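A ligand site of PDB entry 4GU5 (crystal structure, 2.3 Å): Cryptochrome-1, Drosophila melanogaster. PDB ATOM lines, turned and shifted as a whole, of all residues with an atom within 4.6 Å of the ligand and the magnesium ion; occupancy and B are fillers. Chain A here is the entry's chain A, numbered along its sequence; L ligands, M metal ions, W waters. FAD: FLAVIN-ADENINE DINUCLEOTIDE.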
ATOM      1  N   ARG A 237     -24.795  -3.100  21.607  1.00  0.00           N
ATOM      2  CA  ARG A 237     -25.922  -2.265  21.951  1.00  0.00           C
ATOM      3  C   ARG A 237     -27.141  -2.678  21.134  1.00  0.00           C
ATOM      4  O   ARG A 237     -28.240  -2.832  21.660  1.00  0.00           O
ATOM      5  CB  ARG A 237     -25.584  -0.791  21.715  1.00  0.00           C
ATOM      6  CG  ARG A 237     -26.768   0.109  22.007  1.00  0.00           C
ATOM      7  CD  ARG A 237     -26.961   0.301  23.491  1.00  0.00           C
ATOM      8  NE  ARG A 237     -26.628   1.666  23.822  1.00  0.00           N
ATOM      9  CZ  ARG A 237     -27.513   2.587  24.180  1.00  0.00           C
ATOM     10  NH1 ARG A 237     -28.801   2.265  24.291  1.00  0.00           N
ATOM     11  NH2 ARG A 237     -27.099   3.807  24.454  1.00  0.00           N
ATOM     12  N   LYS A 264     -19.304   0.119  28.510  1.00  0.00           N
ATOM     13  CA  LYS A 264     -20.208  -0.131  27.385  1.00  0.00           C
ATOM     14  C   LYS A 264     -20.744   1.138  26.746  1.00  0.00           C
ATOM     15  O   LYS A 264     -21.468   1.070  25.738  1.00  0.00           O
ATOM     16  CB  LYS A 264     -21.393  -1.009  27.810  1.00  0.00           C
ATOM     17  CG  LYS A 264     -21.043  -2.450  28.166  1.00  0.00           C
ATOM     18  CD  LYS A 264     -20.736  -3.273  26.921  1.00  0.00           C
ATOM     19  CE  LYS A 264     -20.195  -4.656  27.282  1.00  0.00           C
ATOM     20  NZ  LYS A 264     -18.786  -4.623  27.801  1.00  0.00           N
ATOM     21  N   SER A 265     -20.426   2.298  27.319  1.00  0.00           N
ATOM     22  CA  SER A 265     -20.827   3.561  26.744  1.00  0.00           C
ATOM     23  C   SER A 265     -20.030   3.856  25.471  1.00  0.00           C
ATOM     24  O   SER A 265     -18.868   3.506  25.372  1.00  0.00           O
ATOM     25  CB  SER A 265     -20.592   4.698  27.742  1.00  0.00           C
ATOM     26  OG  SER A 265     -20.878   5.963  27.169  1.00  0.00           O
ATOM     27  N   MET A 266     -20.672   4.520  24.529  1.00  0.00           N
ATOM     28  CA  MET A 266     -19.992   4.972  23.330  1.00  0.00           C
ATOM     29  C   MET A 266     -19.772   6.487  23.309  1.00  0.00           C
ATOM     30  O   MET A 266     -19.493   7.066  22.259  1.00  0.00           O
ATOM     31  CB  MET A 266     -20.788   4.546  22.108  1.00  0.00           C
ATOM     32  CG  MET A 266     -20.778   3.054  21.927  1.00  0.00           C
ATOM     33  SD  MET A 266     -21.960   2.503  20.700  1.00  0.00           S
ATOM     34  CE  MET A 266     -23.522   2.777  21.559  1.00  0.00           C
ATOM     35  N   SER A 267     -19.877   7.138  24.451  1.00  0.00           N
ATOM     36  CA  SER A 267     -19.813   8.598  24.503  1.00  0.00           C
ATOM     37  C   SER A 267     -18.468   9.156  23.996  1.00  0.00           C
ATOM     38  O   SER A 267     -18.425  10.135  23.250  1.00  0.00           O
ATOM     39  CB  SER A 267     -20.141   9.118  25.906  1.00  0.00           C
ATOM     40  OG  SER A 267     -19.158   8.748  26.848  1.00  0.00           O
ATOM     41  N   LEU A 270     -18.061   8.651  20.277  1.00  0.00           N
ATOM     42  CA  LEU A 270     -18.826   9.654  19.531  1.00  0.00           C
ATOM     43  C   LEU A 270     -18.091  10.964  19.566  1.00  0.00           C
ATOM     44  O   LEU A 270     -18.148  11.732  18.605  1.00  0.00           O
ATOM     45  CB  LEU A 270     -20.246   9.816  20.118  1.00  0.00           C
ATOM     46  CG  LEU A 270     -21.166   8.602  19.924  1.00  0.00           C
ATOM     47  CD1 LEU A 270     -22.354   8.673  20.864  1.00  0.00           C
ATOM     48  CD2 LEU A 270     -21.645   8.529  18.490  1.00  0.00           C
ATOM     49  N   GLN A 311     -31.176  10.418  22.590  1.00  0.00           N
ATOM     50  CA  GLN A 311     -29.938  10.765  23.251  1.00  0.00           C
ATOM     51  C   GLN A 311     -29.039  11.502  22.252  1.00  0.00           C
ATOM     52  O   GLN A 311     -28.330  12.441  22.623  1.00  0.00           O
ATOM     53  CB  GLN A 311     -29.251   9.528  23.816  1.00  0.00           C
ATOM     54  CG  GLN A 311     -30.091   8.781  24.869  1.00  0.00           C
ATOM     55  CD  GLN A 311     -30.436   9.649  26.075  1.00  0.00           C
ATOM     56  OE1 GLN A 311     -31.349  10.463  26.018  1.00  0.00           O
ATOM     57  NE2 GLN A 311     -29.691   9.469  27.177  1.00  0.00           N
ATOM     58  N   LEU A 312     -29.105  11.103  20.988  1.00  0.00           N
ATOM     59  CA  LEU A 312     -28.230  11.684  19.997  1.00  0.00           C
ATOM     60  C   LEU A 312     -28.653  13.119  19.706  1.00  0.00           C
ATOM     61  O   LEU A 312     -27.839  13.965  19.294  1.00  0.00           O
ATOM     62  CB  LEU A 312     -28.200  10.833  18.705  1.00  0.00           C
ATOM     63  CG  LEU A 312     -27.703   9.391  18.901  1.00  0.00           C
ATOM     64  CD1 LEU A 312     -27.437   8.682  17.572  1.00  0.00           C
ATOM     65  CD2 LEU A 312     -26.443   9.317  19.772  1.00  0.00           C
ATOM     66  N   TRP A 314     -29.811  15.164  22.069  1.00  0.00           N
ATOM     67  CA  TRP A 314     -29.299  16.002  23.143  1.00  0.00           C
ATOM     68  C   TRP A 314     -27.914  16.467  22.746  1.00  0.00           C
ATOM     69  O   TRP A 314     -27.585  17.643  22.850  1.00  0.00           O
ATOM     70  CB  TRP A 314     -29.267  15.244  24.468  1.00  0.00           C
ATOM     71  CG  TRP A 314     -30.582  15.222  25.181  1.00  0.00           C
ATOM     72  CD1 TRP A 314     -31.536  14.242  25.120  1.00  0.00           C
ATOM     73  CD2 TRP A 314     -31.103  16.238  26.031  1.00  0.00           C
ATOM     74  NE1 TRP A 314     -32.614  14.584  25.912  1.00  0.00           N
ATOM     75  CE2 TRP A 314     -32.377  15.807  26.473  1.00  0.00           C
ATOM     76  CE3 TRP A 314     -30.623  17.473  26.478  1.00  0.00           C
ATOM     77  CZ2 TRP A 314     -33.156  16.563  27.332  1.00  0.00           C
ATOM     78  CZ3 TRP A 314     -31.387  18.213  27.328  1.00  0.00           C
ATOM     79  CH2 TRP A 314     -32.648  17.761  27.753  1.00  0.00           C
ATOM     80  N   ARG A 315     -27.104  15.521  22.297  1.00  0.00           N
ATOM     81  CA  ARG A 315     -25.775  15.827  21.808  1.00  0.00           C
ATOM     82  C   ARG A 315     -25.876  16.944  20.778  1.00  0.00           C
ATOM     83  O   ARG A 315     -25.280  18.012  20.936  1.00  0.00           O
ATOM     84  CB  ARG A 315     -25.143  14.570  21.190  1.00  0.00           C
ATOM     85  CG  ARG A 315     -23.701  14.736  20.699  1.00  0.00           C
ATOM     86  CD  ARG A 315     -23.160  13.421  20.115  1.00  0.00           C
ATOM     87  NE  ARG A 315     -21.852  13.572  19.479  1.00  0.00           N
ATOM     88  CZ  ARG A 315     -21.668  13.816  18.180  1.00  0.00           C
ATOM     89  NH1 ARG A 315     -22.700  13.935  17.352  1.00  0.00           N
ATOM     90  NH2 ARG A 315     -20.445  13.925  17.703  1.00  0.00           N
ATOM     91  N   PHE A 318     -26.795  20.684  22.140  1.00  0.00           N
ATOM     92  CA  PHE A 318     -25.714  21.447  22.715  1.00  0.00           C
ATOM     93  C   PHE A 318     -24.641  21.802  21.675  1.00  0.00           C
ATOM     94  O   PHE A 318     -24.184  22.936  21.617  1.00  0.00           O
ATOM     95  CB  PHE A 318     -25.078  20.654  23.848  1.00  0.00           C
ATOM     96  CG  PHE A 318     -25.985  20.486  25.039  1.00  0.00           C
ATOM     97  CD1 PHE A 318     -26.475  21.591  25.717  1.00  0.00           C
ATOM     98  CD2 PHE A 318     -26.305  19.220  25.502  1.00  0.00           C
ATOM     99  CE1 PHE A 318     -27.287  21.448  26.820  1.00  0.00           C
ATOM    100  CE2 PHE A 318     -27.111  19.056  26.610  1.00  0.00           C
ATOM    101  CZ  PHE A 318     -27.610  20.178  27.274  1.00  0.00           C
ATOM    102  N   TRP A 375     -14.677   8.490  33.263  1.00  0.00           N
ATOM    103  CA  TRP A 375     -16.077   8.389  32.876  1.00  0.00           C
ATOM    104  C   TRP A 375     -16.986   8.285  34.089  1.00  0.00           C
ATOM    105  O   TRP A 375     -16.687   7.551  35.016  1.00  0.00           O
ATOM    106  CB  TRP A 375     -16.303   7.199  31.938  1.00  0.00           C
ATOM    107  CG  TRP A 375     -17.638   7.192  31.215  1.00  0.00           C
ATOM    108  CD1 TRP A 375     -17.928   7.752  29.997  1.00  0.00           C
ATOM    109  CD2 TRP A 375     -18.854   6.566  31.657  1.00  0.00           C
ATOM    110  NE1 TRP A 375     -19.243   7.528  29.664  1.00  0.00           N
ATOM    111  CE2 TRP A 375     -19.836   6.806  30.663  1.00  0.00           C
ATOM    112  CE3 TRP A 375     -19.213   5.842  32.802  1.00  0.00           C
ATOM    113  CZ2 TRP A 375     -21.158   6.339  30.780  1.00  0.00           C
ATOM    114  CZ3 TRP A 375     -20.525   5.372  32.917  1.00  0.00           C
ATOM    115  CH2 TRP A 375     -21.473   5.634  31.907  1.00  0.00           C
ATOM    116  N   LEU A 376     -18.086   9.026  34.076  1.00  0.00           N
ATOM    117  CA  LEU A 376     -19.105   8.945  35.113  1.00  0.00           C
ATOM    118  C   LEU A 376     -20.433   8.751  34.444  1.00  0.00           C
ATOM    119  O   LEU A 376     -20.712   9.350  33.406  1.00  0.00           O
ATOM    120  CB  LEU A 376     -19.194  10.240  35.911  1.00  0.00           C
ATOM    121  CG  LEU A 376     -18.055  10.514  36.866  1.00  0.00           C
ATOM    122  CD1 LEU A 376     -18.165  11.939  37.437  1.00  0.00           C
ATOM    123  CD2 LEU A 376     -18.121   9.480  37.955  1.00  0.00           C
ATOM    124  N   HIS A 377     -21.254   7.906  35.044  1.00  0.00           N
ATOM    125  CA  HIS A 377     -22.626   7.747  34.605  1.00  0.00           C
ATOM    126  C   HIS A 377     -23.324   9.101  34.625  1.00  0.00           C
ATOM    127  O   HIS A 377     -22.959  10.002  35.388  1.00  0.00           O
ATOM    128  CB  HIS A 377     -23.347   6.772  35.520  1.00  0.00           C
ATOM    129  CG  HIS A 377     -24.727   6.427  35.051  1.00  0.00           C
ATOM    130  ND1 HIS A 377     -25.834   7.164  35.402  1.00  0.00           N
ATOM    131  CD2 HIS A 377     -25.174   5.420  34.261  1.00  0.00           C
ATOM    132  CE1 HIS A 377     -26.901   6.623  34.842  1.00  0.00           C
ATOM    133  NE2 HIS A 377     -26.529   5.563  34.147  1.00  0.00           N
ATOM    134  N   HIS A 378     -24.335   9.240  33.773  1.00  0.00           N
ATOM    135  CA  HIS A 378     -24.999  10.511  33.628  1.00  0.00           C
ATOM    136  C   HIS A 378     -25.529  11.027  34.967  1.00  0.00           C
ATOM    137  O   HIS A 378     -25.490  12.217  35.231  1.00  0.00           O
ATOM    138  CB  HIS A 378     -26.083  10.438  32.544  1.00  0.00           C
ATOM    139  CG  HIS A 378     -26.876  11.690  32.407  1.00  0.00           C
ATOM    140  ND1 HIS A 378     -26.381  12.814  31.772  1.00  0.00           N
ATOM    141  CD2 HIS A 378     -28.102  12.028  32.857  1.00  0.00           C
ATOM    142  CE1 HIS A 378     -27.281  13.778  31.823  1.00  0.00           C
ATOM    143  NE2 HIS A 378     -28.344  13.322  32.480  1.00  0.00           N
ATOM    144  N   ARG A 381     -22.596  12.508  37.132  1.00  0.00           N
ATOM    145  CA  ARG A 381     -22.309  13.804  36.568  1.00  0.00           C
ATOM    146  C   ARG A 381     -23.308  14.835  37.070  1.00  0.00           C
ATOM    147  O   ARG A 381     -22.925  15.887  37.566  1.00  0.00           O
ATOM    148  CB  ARG A 381     -22.324  13.738  35.040  1.00  0.00           C
ATOM    149  CG  ARG A 381     -21.226  12.869  34.464  1.00  0.00           C
ATOM    150  CD  ARG A 381     -21.104  13.052  32.963  1.00  0.00           C
ATOM    151  NE  ARG A 381     -20.635  11.839  32.308  1.00  0.00           N
ATOM    152  CZ  ARG A 381     -19.999  11.820  31.135  1.00  0.00           C
ATOM    153  NH1 ARG A 381     -19.770  12.944  30.474  1.00  0.00           N
ATOM    154  NH2 ARG A 381     -19.608  10.662  30.612  1.00  0.00           N
ATOM    155  N   ASN A 382     -24.594  14.527  36.946  1.00  0.00           N
ATOM    156  CA  ASN A 382     -25.667  15.340  37.557  1.00  0.00           C
ATOM    157  C   ASN A 382     -25.365  15.717  38.995  1.00  0.00           C
ATOM    158  O   ASN A 382     -25.353  16.902  39.346  1.00  0.00           O
ATOM    159  CB  ASN A 382     -27.033  14.618  37.537  1.00  0.00           C
ATOM    160  CG  ASN A 382     -27.643  14.574  36.149  1.00  0.00           C
ATOM    161  OD1 ASN A 382     -27.253  15.320  35.262  1.00  0.00           O
ATOM    162  ND2 ASN A 382     -28.609  13.686  35.960  1.00  0.00           N
ATOM    163  N   ALA A 385     -22.294  18.015  39.724  1.00  0.00           N
ATOM    164  CA  ALA A 385     -22.518  19.300  39.116  1.00  0.00           C
ATOM    165  C   ALA A 385     -23.455  20.153  39.961  1.00  0.00           C
ATOM    166  O   ALA A 385     -23.207  21.336  40.183  1.00  0.00           O
ATOM    167  CB  ALA A 385     -23.120  19.115  37.733  1.00  0.00           C
ATOM    168  N   PHE A 404     -13.900  18.932  34.223  1.00  0.00           N
ATOM    169  CA  PHE A 404     -14.397  17.859  33.360  1.00  0.00           C
ATOM    170  C   PHE A 404     -13.664  17.795  32.035  1.00  0.00           C
ATOM    171  O   PHE A 404     -13.478  16.715  31.485  1.00  0.00           O
ATOM    172  CB  PHE A 404     -15.883  18.042  33.048  1.00  0.00           C
ATOM    173  CG  PHE A 404     -16.809  17.475  34.081  1.00  0.00           C
ATOM    174  CD1 PHE A 404     -16.407  17.360  35.394  1.00  0.00           C
ATOM    175  CD2 PHE A 404     -18.067  17.026  33.725  1.00  0.00           C
ATOM    176  CE1 PHE A 404     -17.251  16.854  36.340  1.00  0.00           C
ATOM    177  CE2 PHE A 404     -18.916  16.492  34.682  1.00  0.00           C
ATOM    178  CZ  PHE A 404     -18.498  16.411  35.979  1.00  0.00           C
ATOM    179  N   LEU A 408     -12.557  13.946  31.615  1.00  0.00           N
ATOM    180  CA  LEU A 408     -13.548  13.113  30.931  1.00  0.00           C
ATOM    181  C   LEU A 408     -12.978  12.498  29.661  1.00  0.00           C
ATOM    182  O   LEU A 408     -12.314  13.176  28.878  1.00  0.00           O
ATOM    183  CB  LEU A 408     -14.779  13.930  30.564  1.00  0.00           C
ATOM    184  CG  LEU A 408     -15.828  14.110  31.669  1.00  0.00           C
ATOM    185  CD1 LEU A 408     -16.851  15.127  31.207  1.00  0.00           C
ATOM    186  CD2 LEU A 408     -16.481  12.772  32.061  1.00  0.00           C
ATOM    187  N   ASP A 410     -14.832  11.570  27.249  1.00  0.00           N
ATOM    188  CA  ASP A 410     -15.590  12.236  26.184  1.00  0.00           C
ATOM    189  C   ASP A 410     -15.273  13.758  26.113  1.00  0.00           C
ATOM    190  O   ASP A 410     -14.416  14.166  25.308  1.00  0.00           O
ATOM    191  CB  ASP A 410     -17.104  11.907  26.216  1.00  0.00           C
ATOM    192  CG  ASP A 410     -17.699  11.916  27.622  1.00  0.00           C
ATOM    193  OD1 ASP A 410     -17.468  12.885  28.363  1.00  0.00           O
ATOM    194  OD2 ASP A 410     -18.424  10.959  27.984  1.00  0.00           O
ATOM    195  N   ALA A 411     -15.933  14.566  26.932  1.00  0.00           N
ATOM    196  CA  ALA A 411     -15.557  15.970  27.106  1.00  0.00           C
ATOM    197  C   ALA A 411     -15.633  16.834  25.863  1.00  0.00           C
ATOM    198  O   ALA A 411     -14.715  17.574  25.582  1.00  0.00           O
ATOM    199  CB  ALA A 411     -14.172  16.083  27.734  1.00  0.00           C
ATOM    200  N   ASP A 412     -16.716  16.766  25.116  1.00  0.00           N
ATOM    201  CA  ASP A 412     -16.925  17.693  24.030  1.00  0.00           C
ATOM    202  C   ASP A 412     -16.984  19.068  24.660  1.00  0.00           C
ATOM    203  O   ASP A 412     -17.603  19.260  25.700  1.00  0.00           O
ATOM    204  CB  ASP A 412     -18.236  17.403  23.292  1.00  0.00           C
ATOM    205  CG  ASP A 412     -18.346  15.958  22.798  1.00  0.00           C
ATOM    206  OD1 ASP A 412     -17.985  15.011  23.544  1.00  0.00           O
ATOM    207  OD2 ASP A 412     -18.812  15.761  21.657  1.00  0.00           O
ATOM    208  N   VAL A 415     -20.840  20.137  24.339  1.00  0.00           N
ATOM    209  CA  VAL A 415     -21.750  19.288  25.085  1.00  0.00           C
ATOM    210  C   VAL A 415     -21.561  19.499  26.580  1.00  0.00           C
ATOM    211  O   VAL A 415     -22.532  19.665  27.330  1.00  0.00           O
ATOM    212  CB  VAL A 415     -21.570  17.803  24.747  1.00  0.00           C
ATOM    213  CG1 VAL A 415     -22.431  16.954  25.644  1.00  0.00           C
ATOM    214  CG2 VAL A 415     -21.904  17.560  23.302  1.00  0.00           C
ATOM    215  N   CYS A 416     -20.303  19.540  27.005  1.00  0.00           N
ATOM    216  CA  CYS A 416     -20.004  19.614  28.422  1.00  0.00           C
ATOM    217  C   CYS A 416     -20.425  20.960  28.995  1.00  0.00           C
ATOM    218  O   CYS A 416     -20.986  21.009  30.082  1.00  0.00           O
ATOM    219  CB  CYS A 416     -18.511  19.374  28.676  1.00  0.00           C
ATOM    220  SG  CYS A 416     -18.102  18.974  30.396  1.00  0.00           S
ATOM    221  N   ASN A 419     -24.331  21.044  29.106  1.00  0.00           N
ATOM    222  CA  ASN A 419     -24.800  20.354  30.290  1.00  0.00           C
ATOM    223  C   ASN A 419     -24.539  21.114  31.580  1.00  0.00           C
ATOM    224  O   ASN A 419     -25.425  21.208  32.431  1.00  0.00           O
ATOM    225  CB  ASN A 419     -24.259  18.930  30.359  1.00  0.00           C
ATOM    226  CG  ASN A 419     -24.981  18.033  29.406  1.00  0.00           C
ATOM    227  OD1 ASN A 419     -26.071  17.567  29.702  1.00  0.00           O
ATOM    228  ND2 ASN A 419     -24.421  17.835  28.220  1.00  0.00           N
ATOM    229  N   TRP A 420     -23.345  21.675  31.727  1.00  0.00           N
ATOM    230  CA  TRP A 420     -23.087  22.494  32.920  1.00  0.00           C
ATOM    231  C   TRP A 420     -24.062  23.676  33.077  1.00  0.00           C
ATOM    232  O   TRP A 420     -24.583  23.901  34.155  1.00  0.00           O
ATOM    233  CB  TRP A 420     -21.641  22.978  32.949  1.00  0.00           C
ATOM    234  CG  TRP A 420     -20.735  22.001  33.571  1.00  0.00           C
ATOM    235  CD1 TRP A 420     -19.893  21.160  32.933  1.00  0.00           C
ATOM    236  CD2 TRP A 420     -20.587  21.757  34.977  1.00  0.00           C
ATOM    237  NE1 TRP A 420     -19.209  20.390  33.847  1.00  0.00           N
ATOM    238  CE2 TRP A 420     -19.612  20.746  35.110  1.00  0.00           C
ATOM    239  CE3 TRP A 420     -21.181  22.282  36.121  1.00  0.00           C
ATOM    240  CZ2 TRP A 420     -19.209  20.252  36.350  1.00  0.00           C
ATOM    241  CZ3 TRP A 420     -20.778  21.788  37.362  1.00  0.00           C
ATOM    242  CH2 TRP A 420     -19.812  20.773  37.455  1.00  0.00           C
ATOM    243  N   VAL A 423     -27.902  22.329  33.694  1.00  0.00           N
ATOM    244  CA  VAL A 423     -28.101  21.848  35.048  1.00  0.00           C
ATOM    245  C   VAL A 423     -28.083  22.977  36.074  1.00  0.00           C
ATOM    246  O   VAL A 423     -28.971  23.063  36.929  1.00  0.00           O
ATOM    247  CB  VAL A 423     -26.968  20.869  35.433  1.00  0.00           C
ATOM    248  CG1 VAL A 423     -26.896  20.711  36.939  1.00  0.00           C
ATOM    249  CG2 VAL A 423     -27.148  19.515  34.729  1.00  0.00           C
ATOM    250  N   PHE A 534     -34.261  13.857  32.488  1.00  0.00           N
ATOM    251  CA  PHE A 534     -32.841  14.227  32.522  1.00  0.00           C
ATOM    252  C   PHE A 534     -32.135  13.752  33.795  1.00  0.00           C
ATOM    253  O   PHE A 534     -31.011  13.250  33.738  1.00  0.00           O
ATOM    254  CB  PHE A 534     -32.674  15.737  32.386  1.00  0.00           C
ATOM    255  CG  PHE A 534     -31.250  16.196  32.156  1.00  0.00           C
ATOM    256  CD1 PHE A 534     -30.370  16.350  33.222  1.00  0.00           C
ATOM    257  CD2 PHE A 534     -30.807  16.539  30.884  1.00  0.00           C
ATOM    258  CE1 PHE A 534     -29.079  16.805  33.008  1.00  0.00           C
ATOM    259  CE2 PHE A 534     -29.507  16.992  30.668  1.00  0.00           C
ATOM    260  CZ  PHE A 534     -28.644  17.123  31.725  1.00  0.00           C
HETATM  261  PA  FAD L   1     -26.603   7.167  26.503  1.00  0.00           P
HETATM  262  O1A FAD L   1     -26.285   5.771  26.117  1.00  0.00           O
HETATM  263  O2A FAD L   1     -27.891   7.341  27.335  1.00  0.00           O
HETATM  264  O5B FAD L   1     -26.708   8.007  25.189  1.00  0.00           O
HETATM  265  C5B FAD L   1     -25.831   7.847  24.090  1.00  0.00           C
HETATM  266  C4B FAD L   1     -25.216   9.090  23.556  1.00  0.00           C
HETATM  267  O4B FAD L   1     -26.133  10.139  23.460  1.00  0.00           O
HETATM  268  C3B FAD L   1     -24.241   9.569  24.492  1.00  0.00           C
HETATM  269  O3B FAD L   1     -23.062   8.745  24.360  1.00  0.00           O
HETATM  270  C2B FAD L   1     -24.088  10.913  24.101  1.00  0.00           C
HETATM  271  O2B FAD L   1     -23.358  10.991  22.912  1.00  0.00           O
HETATM  272  C1B FAD L   1     -25.476  11.309  23.817  1.00  0.00           C
HETATM  273  N9A FAD L   1     -26.025  11.923  25.038  1.00  0.00           N
HETATM  274  C8A FAD L   1     -26.656  11.298  26.045  1.00  0.00           C
HETATM  275  N7A FAD L   1     -26.966  12.201  27.000  1.00  0.00           N
HETATM  276  C5A FAD L   1     -26.532  13.409  26.603  1.00  0.00           C
HETATM  277  C6A FAD L   1     -26.579  14.682  27.146  1.00  0.00           C
HETATM  278  N6A FAD L   1     -27.170  14.951  28.414  1.00  0.00           N
HETATM  279  N1A FAD L   1     -26.014  15.685  26.482  1.00  0.00           N
HETATM  280  C2A FAD L   1     -25.439  15.470  25.286  1.00  0.00           C
HETATM  281  N3A FAD L   1     -25.391  14.264  24.719  1.00  0.00           N
HETATM  282  C4A FAD L   1     -25.919  13.221  25.355  1.00  0.00           C
HETATM  283  N1  FAD L   1     -21.724  13.928  27.327  1.00  0.00           N
HETATM  284  C2  FAD L   1     -20.724  13.905  26.430  1.00  0.00           C
HETATM  285  O2  FAD L   1     -20.859  13.099  25.320  1.00  0.00           O
HETATM  286  N3  FAD L   1     -19.618  14.653  26.599  1.00  0.00           N
HETATM  287  C4  FAD L   1     -19.514  15.448  27.667  1.00  0.00           C
HETATM  288  O4  FAD L   1     -18.388  16.206  27.816  1.00  0.00           O
HETATM  289  C4X FAD L   1     -20.527  15.512  28.607  1.00  0.00           C
HETATM  290  N5  FAD L   1     -20.424  16.291  29.692  1.00  0.00           N
HETATM  291  C5X FAD L   1     -21.446  16.299  30.599  1.00  0.00           C
HETATM  292  C6  FAD L   1     -21.366  17.122  31.729  1.00  0.00           C
HETATM  293  C7  FAD L   1     -22.396  17.164  32.660  1.00  0.00           C
HETATM  294  C7M FAD L   1     -22.273  18.088  33.896  1.00  0.00           C
HETATM  295  C8  FAD L   1     -23.529  16.368  32.472  1.00  0.00           C
HETATM  296  C8M FAD L   1     -24.664  16.414  33.506  1.00  0.00           C
HETATM  297  C9  FAD L   1     -23.616  15.557  31.339  1.00  0.00           C
HETATM  298  C9A FAD L   1     -22.574  15.516  30.416  1.00  0.00           C
HETATM  299  N10 FAD L   1     -22.652  14.718  29.321  1.00  0.00           N
HETATM  300  C10 FAD L   1     -21.646  14.726  28.422  1.00  0.00           C
HETATM  301  C1' FAD L   1     -23.839  13.908  29.020  1.00  0.00           C
HETATM  302  C2' FAD L   1     -24.132  12.487  29.378  1.00  0.00           C
HETATM  303  O2' FAD L   1     -23.983  12.346  30.879  1.00  0.00           O
HETATM  304  C3' FAD L   1     -23.221  11.478  28.705  1.00  0.00           C
HETATM  305  O3' FAD L   1     -23.315  11.581  27.324  1.00  0.00           O
HETATM  306  C4' FAD L   1     -23.697  10.085  29.113  1.00  0.00           C
HETATM  307  O4' FAD L   1     -23.361   9.840  30.404  1.00  0.00           O
HETATM  308  C5' FAD L   1     -23.057   8.982  28.284  1.00  0.00           C
HETATM  309  O5' FAD L   1     -23.306   7.682  28.664  1.00  0.00           O
HETATM  310  P   FAD L   1     -24.089   6.800  27.590  1.00  0.00           P
HETATM  311  O1P FAD L   1     -23.291   6.732  26.282  1.00  0.00           O
HETATM  312  O2P FAD L   1     -24.365   5.438  28.185  1.00  0.00           O
HETATM  313  O3P FAD L   1     -25.348   7.706  27.352  1.00  0.00           O
HETATM  314 MG    MG M   1     -23.385   4.942  24.450  1.00  0.00          MG
HETATM  315  O   HOH W   1     -25.005   7.540  31.363  1.00  0.00           O
HETATM  316  O   HOH W   2     -27.409   8.390  30.138  1.00  0.00           O
HETATM  317  O   HOH W   3     -24.711   4.716  31.046  1.00  0.00           O
HETATM  318  O   HOH W   4     -23.941   2.766  27.757  1.00  0.00           O
HETATM  319  O   HOH W   5     -30.032   5.711  26.884  1.00  0.00           O
HETATM  320  O   HOH W   6     -20.461  11.645  23.060  1.00  0.00           O
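OG of Ser 267 is in hydrogen-bond range of OD2 of Asp 410 (2.6 Å).
NH2 of Arg 381 lies within salt-bridge range of OD2 of Asp 410.
The side-chain hydroxyl (OG) of Ser 265 lies within hydrogen-bond range of the backbone NH (N) of Ser 267, at 3.1 Å.
The side-chain hydroxyl (OG) of Ser 267 lies within hydrogen-bond range of the indole nitrogen (NE1) of Trp 375 (3.1 Å).
The backbone carbonyl oxygen (O) of Val 415 lies within hydrogen-bond range of the side-chain amide nitrogen (ND2) of Asn 419, 2.8 Å away.
The guanidinium group (NH2) of Arg 315 lies within hydrogen-bond range of the backbone carbonyl oxygen (O) of Leu 270, at 3.3 Å.
NE1 of Trp 375 lies within hydrogen-bond range of OG of Ser 265 (3.4 Å).
The backbone carbonyl oxygen (O) of Leu 376 is in hydrogen-bond range of the guanidinium group (NE) of Arg 381 (2.7 Å).
Arg 237 touches the magnesium ion.
C of Ser 265 touches the magnesium ion, at 3.7 Å.
The magnesium ion is bound by O1P of the ligand (2.6 Å).
Slightly farther from the magnesium ion lies N of Met 266 (2.7 Å).
Residues that only touch the ligand: Leu 270 (3.3 Å), Ser 267 (3.3 Å), Trp 375 (3.3 Å), Asn 382 (3.3 Å), Val 415 (3.4 Å), Phe 318 (3.5 Å), Trp 314 (3.7 Å), Leu 312 (3.8 Å), Phe 404 (3.8 Å), Trp 420 (3.8 Å), Phe 534 (3.8 Å) and Leu 408 (3.9 Å).
Hydrophobic or aromatic side chains that line the ligand: Leu 270, Leu 312, Trp 314, Phe 318, Trp 375, His 378, Phe 404, Leu 408, Val 415, Trp 420 and Phe 534.
24 residues have an atom within 4 Å of the ligand: Arg 237, Ser 265, Met 266, Ser 267, Leu 270, Gln 311, Leu 312, Trp 314, Arg 315, Phe 318, Trp 375, His 378, Arg 381, Asn 382, Phe 404, Leu 408, Asp 410, Ala 411, Asp 412, Val 415, Cys 416, Asn 419, Trp 420 and Phe 534.
The nearest printed residue that does not touch the ligand is Leu 376 (4.03 Å).
Water W6 lies within hydrogen-bond range of O of Ser 267 (2.5 Å) and O2 of the ligand (2.7 Å).
Water W1 bridges O4' of the ligand (3.0 Å) and N of His 378 (3.0 Å).
The guanidinium group of Arg 381 lies close to a nitrogen (N5) of the ligand, 3.5 Å away.
SG of Cys 416 lies close to N5 of the ligand, 3.6 Å away.
The backbone NH of Asp 412 is in hydrogen-bond range of an oxygen (O4) of the ligand (3.2 Å).
The backbone NH (N) of Arg 315 sits at hydrogen-bond distance from a nitrogen (N3A) of the ligand (3.2 Å).
An oxygen (O1A) of the ligand lies within salt-bridge range of the guanidinium group (NH2) of Arg 237, 2.7 Å away.
A ring nitrogen (ND1) of His 378 sits at hydrogen-bond distance from an oxygen (O2') of the ligand.
The side-chain hydroxyl (OG) of Ser 265 lies within hydrogen-bond range of an oxygen (O5') of the ligand, 3.3 Å away.
N of Ala 411 sits close to O4 of the ligand.
O2A of the ligand sits at hydrogen-bond distance from NE2 of Gln 311, at 2.8 Å.
A nitrogen (N6A) of the ligand sits at hydrogen-bond distance from the side-chain amide oxygen (OD1) of Asn 419, at 3.1 Å.
The side-chain carboxylate of Asp 410 lies within hydrogen-bond range of a nitrogen (N3) of the ligand (3.3 Å).
N3 of the ligand is in hydrogen-bond range of OD1 of Asp 412, 3.5 Å away.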
